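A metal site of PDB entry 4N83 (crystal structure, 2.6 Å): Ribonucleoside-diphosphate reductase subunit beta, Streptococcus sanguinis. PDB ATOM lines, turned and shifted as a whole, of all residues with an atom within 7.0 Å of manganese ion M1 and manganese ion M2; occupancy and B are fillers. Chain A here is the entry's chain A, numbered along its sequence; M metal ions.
OE2 of Glu 191 sits close to ND1 of His 100.
NE2 of His 100 sits close to O of Met 96, 3.4 Å away.
The side-chain carboxylate (OD2) of Asp 66 lies within hydrogen-bond range of the side-chain hydroxyl (OH) of Tyr 104 (2.7 Å).
A ring nitrogen (ND1) of His 100 lies close to the side-chain carboxylate of Glu 97, at 3.5 Å.
A ring nitrogen (ND1) of His 194 sits close to the side-chain carboxylate (OE1) of Glu 191 (3.1 Å).
OE1 of Glu 157 sits close to OE1 of Gln 69 (2.9 Å).
The side-chain carboxylate (OD2) of Asp 190 is in hydrogen-bond range of a ring nitrogen (NE2) of His 100 (3.2 Å).
O of Asp 190 lies close to ND1 of His 194 (3.4 Å).
His 194 touches manganese ion M2 (ND1 to MN, 3.0 Å).
Along chain A the residues within 4 Å of manganese ion M2 span positions 97 to 194.
Manganese ion M1 is bound by the side-chain carboxylate (OD1) of Asp 66 (2.1 Å).
OE2 of Glu 191 binds manganese ion M1 (2.2 Å).
Manganese ion M1 is bound by the side-chain carboxylate (OE1) of Glu 97 (2.2 Å).
The side-chain carboxylate (OE2) of Glu 157 binds manganese ion M1 (2.4 Å).
Slightly farther from manganese ion M1 lies ND1 of His 100 (2.9 Å).
Manganese ion M2 is bound by OE1 of Glu 157 (2.0 Å), OE2 of Glu 97 (2.2 Å) and OE1 of Glu 191 (2.4 Å).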
ATOM      1  N   LEU A  62      -1.611  -5.048 -19.438  1.00  0.00           N
ATOM      2  CA  LEU A  62      -2.701  -5.974 -19.147  1.00  0.00           C
ATOM      3  C   LEU A  62      -3.997  -5.214 -18.807  1.00  0.00           C
ATOM      4  O   LEU A  62      -5.091  -5.680 -19.126  1.00  0.00           O
ATOM      5  CB  LEU A  62      -2.325  -6.885 -17.977  1.00  0.00           C
ATOM      6  CG  LEU A  62      -1.110  -7.804 -18.170  1.00  0.00           C
ATOM      7  CD1 LEU A  62      -0.682  -8.392 -16.834  1.00  0.00           C
ATOM      8  CD2 LEU A  62      -1.402  -8.893 -19.186  1.00  0.00           C
ATOM      9  N   LEU A  65      -6.159  -4.769 -21.683  1.00  0.00           N
ATOM     10  CA  LEU A  65      -6.862  -5.969 -22.127  1.00  0.00           C
ATOM     11  C   LEU A  65      -7.964  -6.436 -21.166  1.00  0.00           C
ATOM     12  O   LEU A  65      -8.907  -7.112 -21.589  1.00  0.00           O
ATOM     13  CB  LEU A  65      -5.873  -7.100 -22.360  1.00  0.00           C
ATOM     14  CG  LEU A  65      -4.768  -6.803 -23.384  1.00  0.00           C
ATOM     15  CD1 LEU A  65      -3.680  -7.873 -23.325  1.00  0.00           C
ATOM     16  CD2 LEU A  65      -5.335  -6.683 -24.790  1.00  0.00           C
ATOM     17  N   ASP A  66      -7.856  -6.087 -19.888  1.00  0.00           N
ATOM     18  CA  ASP A  66      -8.946  -6.304 -18.934  1.00  0.00           C
ATOM     19  C   ASP A  66     -10.042  -5.256 -19.118  1.00  0.00           C
ATOM     20  O   ASP A  66     -11.209  -5.497 -18.771  1.00  0.00           O
ATOM     21  CB  ASP A  66      -8.442  -6.324 -17.476  1.00  0.00           C
ATOM     22  CG  ASP A  66      -8.085  -7.724 -16.996  1.00  0.00           C
ATOM     23  OD1 ASP A  66      -8.933  -8.622 -17.078  1.00  0.00           O
ATOM     24  OD2 ASP A  66      -6.947  -7.908 -16.513  1.00  0.00           O
ATOM     25  N   GLN A  69     -11.940  -6.515 -22.276  1.00  0.00           N
ATOM     26  CA  GLN A  69     -12.840  -7.624 -21.963  1.00  0.00           C
ATOM     27  C   GLN A  69     -14.122  -7.162 -21.256  1.00  0.00           C
ATOM     28  O   GLN A  69     -15.220  -7.606 -21.610  1.00  0.00           O
ATOM     29  CB  GLN A  69     -12.133  -8.676 -21.105  1.00  0.00           C
ATOM     30  CG  GLN A  69     -11.095  -9.500 -21.858  1.00  0.00           C
ATOM     31  CD  GLN A  69     -11.709 -10.527 -22.787  1.00  0.00           C
ATOM     32  OE1 GLN A  69     -11.790 -11.702 -22.461  1.00  0.00           O
ATOM     33  NE2 GLN A  69     -12.151 -10.077 -23.951  1.00  0.00           N
ATOM     34  N   VAL A  74     -16.898  -9.430 -23.275  1.00  0.00           N
ATOM     35  CA  VAL A  74     -17.958 -10.312 -22.761  1.00  0.00           C
ATOM     36  C   VAL A  74     -19.307  -9.915 -23.360  1.00  0.00           C
ATOM     37  O   VAL A  74     -20.206 -10.750 -23.493  1.00  0.00           O
ATOM     38  CB  VAL A  74     -18.027 -10.294 -21.224  1.00  0.00           C
ATOM     39  CG1 VAL A  74     -19.089 -11.277 -20.728  1.00  0.00           C
ATOM     40  CG2 VAL A  74     -16.666 -10.639 -20.614  1.00  0.00           C
ATOM     41  N   LEU A  77     -19.594 -11.944 -26.421  1.00  0.00           N
ATOM     42  CA  LEU A  77     -19.823 -13.347 -26.056  1.00  0.00           C
ATOM     43  C   LEU A  77     -21.241 -13.611 -25.562  1.00  0.00           C
ATOM     44  O   LEU A  77     -21.761 -14.722 -25.724  1.00  0.00           O
ATOM     45  CB  LEU A  77     -18.812 -13.786 -24.989  1.00  0.00           C
ATOM     46  CG  LEU A  77     -17.343 -13.843 -25.431  1.00  0.00           C
ATOM     47  CD1 LEU A  77     -16.414 -13.882 -24.227  1.00  0.00           C
ATOM     48  CD2 LEU A  77     -17.099 -15.040 -26.337  1.00  0.00           C
ATOM     49  N   ILE A  93     -19.088 -12.927 -15.168  1.00  0.00           N
ATOM     50  CA  ILE A  93     -17.778 -12.880 -15.821  1.00  0.00           C
ATOM     51  C   ILE A  93     -17.408 -11.432 -16.134  1.00  0.00           C
ATOM     52  O   ILE A  93     -16.307 -10.996 -15.816  1.00  0.00           O
ATOM     53  CB  ILE A  93     -17.741 -13.714 -17.119  1.00  0.00           C
ATOM     54  CG1 ILE A  93     -17.849 -15.214 -16.792  1.00  0.00           C
ATOM     55  CG2 ILE A  93     -16.455 -13.445 -17.895  1.00  0.00           C
ATOM     56  CD1 ILE A  93     -18.227 -16.088 -17.967  1.00  0.00           C
ATOM     57  N   MET A  96     -16.449  -9.315 -13.072  1.00  0.00           N
ATOM     58  CA  MET A  96     -15.116  -9.677 -12.579  1.00  0.00           C
ATOM     59  C   MET A  96     -13.999  -9.172 -13.490  1.00  0.00           C
ATOM     60  O   MET A  96     -12.904  -8.887 -13.017  1.00  0.00           O
ATOM     61  CB  MET A  96     -14.996 -11.198 -12.372  1.00  0.00           C
ATOM     62  CG  MET A  96     -15.835 -11.753 -11.232  1.00  0.00           C
ATOM     63  SD  MET A  96     -15.682 -10.868  -9.666  1.00  0.00           S
ATOM     64  CE  MET A  96     -13.901 -10.870  -9.431  1.00  0.00           C
ATOM     65  N   GLU A  97     -14.279  -9.057 -14.789  1.00  0.00           N
ATOM     66  CA  GLU A  97     -13.318  -8.477 -15.733  1.00  0.00           C
ATOM     67  C   GLU A  97     -13.074  -6.996 -15.430  1.00  0.00           C
ATOM     68  O   GLU A  97     -11.963  -6.493 -15.635  1.00  0.00           O
ATOM     69  CB  GLU A  97     -13.775  -8.645 -17.186  1.00  0.00           C
ATOM     70  CG  GLU A  97     -13.924 -10.096 -17.657  1.00  0.00           C
ATOM     71  CD  GLU A  97     -12.608 -10.836 -17.832  1.00  0.00           C
ATOM     72  OE1 GLU A  97     -11.550 -10.288 -17.454  1.00  0.00           O
ATOM     73  OE2 GLU A  97     -12.632 -11.967 -18.338  1.00  0.00           O
ATOM     74  N   SER A  98     -14.099  -6.302 -14.941  1.00  0.00           N
ATOM     75  CA  SER A  98     -13.951  -4.910 -14.488  1.00  0.00           C
ATOM     76  C   SER A  98     -13.166  -4.813 -13.181  1.00  0.00           C
ATOM     77  O   SER A  98     -12.417  -3.854 -12.980  1.00  0.00           O
ATOM     78  CB  SER A  98     -15.319  -4.227 -14.323  1.00  0.00           C
ATOM     79  OG  SER A  98     -15.773  -3.671 -15.550  1.00  0.00           O
ATOM     80  N   HIS A 100     -10.815  -6.909 -12.352  1.00  0.00           N
ATOM     81  CA  HIS A 100      -9.436  -7.126 -12.800  1.00  0.00           C
ATOM     82  C   HIS A 100      -8.834  -5.842 -13.342  1.00  0.00           C
ATOM     83  O   HIS A 100      -7.675  -5.521 -13.067  1.00  0.00           O
ATOM     84  CB  HIS A 100      -9.380  -8.228 -13.876  1.00  0.00           C
ATOM     85  CG  HIS A 100      -9.889  -9.563 -13.426  1.00  0.00           C
ATOM     86  ND1 HIS A 100     -10.180 -10.583 -14.301  1.00  0.00           N
ATOM     87  CD2 HIS A 100     -10.200 -10.031 -12.191  1.00  0.00           C
ATOM     88  CE1 HIS A 100     -10.624 -11.631 -13.633  1.00  0.00           C
ATOM     89  NE2 HIS A 100     -10.643 -11.316 -12.344  1.00  0.00           N
ATOM     90  N   ALA A 101      -9.625  -5.097 -14.119  1.00  0.00           N
ATOM     91  CA  ALA A 101      -9.173  -3.829 -14.679  1.00  0.00           C
ATOM     92  C   ALA A 101      -8.894  -2.787 -13.595  1.00  0.00           C
ATOM     93  O   ALA A 101      -7.912  -2.049 -13.673  1.00  0.00           O
ATOM     94  CB  ALA A 101     -10.215  -3.295 -15.663  1.00  0.00           C
ATOM     95  N   TYR A 104      -5.507  -3.176 -10.944  1.00  0.00           N
ATOM     96  CA  TYR A 104      -4.228  -2.605 -11.363  1.00  0.00           C
ATOM     97  C   TYR A 104      -4.052  -1.175 -10.854  1.00  0.00           C
ATOM     98  O   TYR A 104      -2.962  -0.779 -10.456  1.00  0.00           O
ATOM     99  CB  TYR A 104      -4.094  -2.608 -12.886  1.00  0.00           C
ATOM    100  CG  TYR A 104      -4.202  -3.974 -13.521  1.00  0.00           C
ATOM    101  CD1 TYR A 104      -3.302  -4.990 -13.204  1.00  0.00           C
ATOM    102  CD2 TYR A 104      -5.199  -4.256 -14.446  1.00  0.00           C
ATOM    103  CE1 TYR A 104      -3.402  -6.245 -13.787  1.00  0.00           C
ATOM    104  CE2 TYR A 104      -5.312  -5.510 -15.035  1.00  0.00           C
ATOM    105  CZ  TYR A 104      -4.403  -6.499 -14.702  1.00  0.00           C
ATOM    106  OH  TYR A 104      -4.507  -7.742 -15.291  1.00  0.00           O
ATOM    107  N   SER A 153     -11.021 -14.904 -26.979  1.00  0.00           N
ATOM    108  CA  SER A 153     -11.062 -14.634 -25.541  1.00  0.00           C
ATOM    109  C   SER A 153     -10.251 -15.660 -24.745  1.00  0.00           C
ATOM    110  O   SER A 153      -9.645 -15.320 -23.721  1.00  0.00           O
ATOM    111  CB  SER A 153     -12.508 -14.606 -25.038  1.00  0.00           C
ATOM    112  OG  SER A 153     -12.572 -14.107 -23.711  1.00  0.00           O
ATOM    113  N   GLU A 157      -6.782 -14.391 -22.606  1.00  0.00           N
ATOM    114  CA  GLU A 157      -6.591 -14.453 -21.161  1.00  0.00           C
ATOM    115  C   GLU A 157      -5.930 -15.729 -20.629  1.00  0.00           C
ATOM    116  O   GLU A 157      -5.417 -15.736 -19.511  1.00  0.00           O
ATOM    117  CB  GLU A 157      -7.926 -14.212 -20.457  1.00  0.00           C
ATOM    118  CG  GLU A 157      -8.536 -12.868 -20.821  1.00  0.00           C
ATOM    119  CD  GLU A 157      -9.827 -12.591 -20.078  1.00  0.00           C
ATOM    120  OE1 GLU A 157     -10.800 -13.354 -20.263  1.00  0.00           O
ATOM    121  OE2 GLU A 157      -9.868 -11.602 -19.316  1.00  0.00           O
ATOM    122  N   PHE A 161      -1.981 -13.332 -21.964  1.00  0.00           N
ATOM    123  CA  PHE A 161      -2.000 -12.577 -20.708  1.00  0.00           C
ATOM    124  C   PHE A 161      -0.772 -12.930 -19.856  1.00  0.00           C
ATOM    125  O   PHE A 161      -0.297 -12.108 -19.071  1.00  0.00           O
ATOM    126  CB  PHE A 161      -3.270 -12.876 -19.901  1.00  0.00           C
ATOM    127  CG  PHE A 161      -4.262 -11.740 -19.864  1.00  0.00           C
ATOM    128  CD1 PHE A 161      -4.678 -11.199 -18.654  1.00  0.00           C
ATOM    129  CD2 PHE A 161      -4.797 -11.218 -21.029  1.00  0.00           C
ATOM    130  CE1 PHE A 161      -5.590 -10.161 -18.608  1.00  0.00           C
ATOM    131  CE2 PHE A 161      -5.721 -10.189 -20.993  1.00  0.00           C
ATOM    132  CZ  PHE A 161      -6.114  -9.646 -19.779  1.00  0.00           C
ATOM    133  N   PHE A 165       1.941 -11.899 -16.654  1.00  0.00           N
ATOM    134  CA  PHE A 165       1.919 -12.622 -15.365  1.00  0.00           C
ATOM    135  C   PHE A 165       3.281 -13.196 -14.956  1.00  0.00           C
ATOM    136  O   PHE A 165       3.501 -13.468 -13.783  1.00  0.00           O
ATOM    137  CB  PHE A 165       0.879 -13.753 -15.384  1.00  0.00           C
ATOM    138  CG  PHE A 165      -0.561 -13.300 -15.449  1.00  0.00           C
ATOM    139  CD1 PHE A 165      -0.994 -12.175 -14.752  1.00  0.00           C
ATOM    140  CD2 PHE A 165      -1.494 -14.024 -16.187  1.00  0.00           C
ATOM    141  CE1 PHE A 165      -2.323 -11.773 -14.806  1.00  0.00           C
ATOM    142  CE2 PHE A 165      -2.821 -13.632 -16.245  1.00  0.00           C
ATOM    143  CZ  PHE A 165      -3.236 -12.502 -15.553  1.00  0.00           C
ATOM    144  N   ILE A 187      -6.587 -13.086  -9.954  1.00  0.00           N
ATOM    145  CA  ILE A 187      -7.007 -12.853 -11.345  1.00  0.00           C
ATOM    146  C   ILE A 187      -6.836 -14.115 -12.190  1.00  0.00           C
ATOM    147  O   ILE A 187      -7.712 -14.453 -12.997  1.00  0.00           O
ATOM    148  CB  ILE A 187      -6.235 -11.679 -11.990  1.00  0.00           C
ATOM    149  CG1 ILE A 187      -6.643 -10.355 -11.330  1.00  0.00           C
ATOM    150  CG2 ILE A 187      -6.486 -11.608 -13.488  1.00  0.00           C
ATOM    151  CD1 ILE A 187      -5.677  -9.209 -11.567  1.00  0.00           C
ATOM    152  N   ASP A 190      -9.562 -16.708 -11.462  1.00  0.00           N
ATOM    153  CA  ASP A 190     -10.797 -16.408 -12.195  1.00  0.00           C
ATOM    154  C   ASP A 190     -10.670 -16.735 -13.681  1.00  0.00           C
ATOM    155  O   ASP A 190     -11.564 -17.349 -14.257  1.00  0.00           O
ATOM    156  CB  ASP A 190     -11.197 -14.940 -12.035  1.00  0.00           C
ATOM    157  CG  ASP A 190     -11.813 -14.638 -10.683  1.00  0.00           C
ATOM    158  OD1 ASP A 190     -12.429 -15.531 -10.074  1.00  0.00           O
ATOM    159  OD2 ASP A 190     -11.671 -13.474 -10.220  1.00  0.00           O
ATOM    160  N   GLU A 191      -9.559 -16.330 -14.278  1.00  0.00           N
ATOM    161  CA  GLU A 191      -9.355 -16.523 -15.717  1.00  0.00           C
ATOM    162  C   GLU A 191      -9.111 -17.984 -16.086  1.00  0.00           C
ATOM    163  O   GLU A 191      -9.395 -18.401 -17.212  1.00  0.00           O
ATOM    164  CB  GLU A 191      -8.211 -15.647 -16.240  1.00  0.00           C
ATOM    165  CG  GLU A 191      -8.477 -14.144 -16.182  1.00  0.00           C
ATOM    166  CD  GLU A 191      -9.734 -13.725 -16.927  1.00  0.00           C
ATOM    167  OE1 GLU A 191     -10.194 -14.473 -17.827  1.00  0.00           O
ATOM    168  OE2 GLU A 191     -10.285 -12.651 -16.622  1.00  0.00           O
ATOM    169  N   HIS A 194     -12.627 -19.093 -16.443  1.00  0.00           N
ATOM    170  CA  HIS A 194     -13.244 -18.479 -17.629  1.00  0.00           C
ATOM    171  C   HIS A 194     -12.849 -19.225 -18.904  1.00  0.00           C
ATOM    172  O   HIS A 194     -13.711 -19.547 -19.723  1.00  0.00           O
ATOM    173  CB  HIS A 194     -12.840 -17.005 -17.758  1.00  0.00           C
ATOM    174  CG  HIS A 194     -13.438 -16.122 -16.713  1.00  0.00           C
ATOM    175  ND1 HIS A 194     -12.849 -14.935 -16.310  1.00  0.00           N
ATOM    176  CD2 HIS A 194     -14.572 -16.243 -15.989  1.00  0.00           C
ATOM    177  CE1 HIS A 194     -13.591 -14.377 -15.377  1.00  0.00           C
ATOM    178  NE2 HIS A 194     -14.647 -15.140 -15.170  1.00  0.00           N
ATOM    179  N   GLY A 195     -11.557 -19.487 -19.049  1.00  0.00           N
ATOM    180  CA  GLY A 195     -11.048 -20.243 -20.190  1.00  0.00           C
ATOM    181  C   GLY A 195     -11.689 -21.607 -20.320  1.00  0.00           C
ATOM    182  O   GLY A 195     -12.083 -22.019 -21.417  1.00  0.00           O
ATOM    183  N   ILE A 198     -15.635 -20.946 -21.208  1.00  0.00           N
ATOM    184  CA  ILE A 198     -15.761 -20.452 -22.579  1.00  0.00           C
ATOM    185  C   ILE A 198     -15.272 -21.521 -23.565  1.00  0.00           C
ATOM    186  O   ILE A 198     -15.893 -21.737 -24.613  1.00  0.00           O
ATOM    187  CB  ILE A 198     -14.969 -19.137 -22.793  1.00  0.00           C
ATOM    188  CG1 ILE A 198     -15.598 -17.996 -21.978  1.00  0.00           C
ATOM    189  CG2 ILE A 198     -14.949 -18.754 -24.270  1.00  0.00           C
ATOM    190  CD1 ILE A 198     -14.743 -16.752 -21.872  1.00  0.00           C
HETATM  191 MN    MN M   1      -9.390 -10.693 -17.131  1.00  0.00          MN
HETATM  192 MN    MN M   2     -12.226 -13.957 -19.053  1.00  0.00          MN
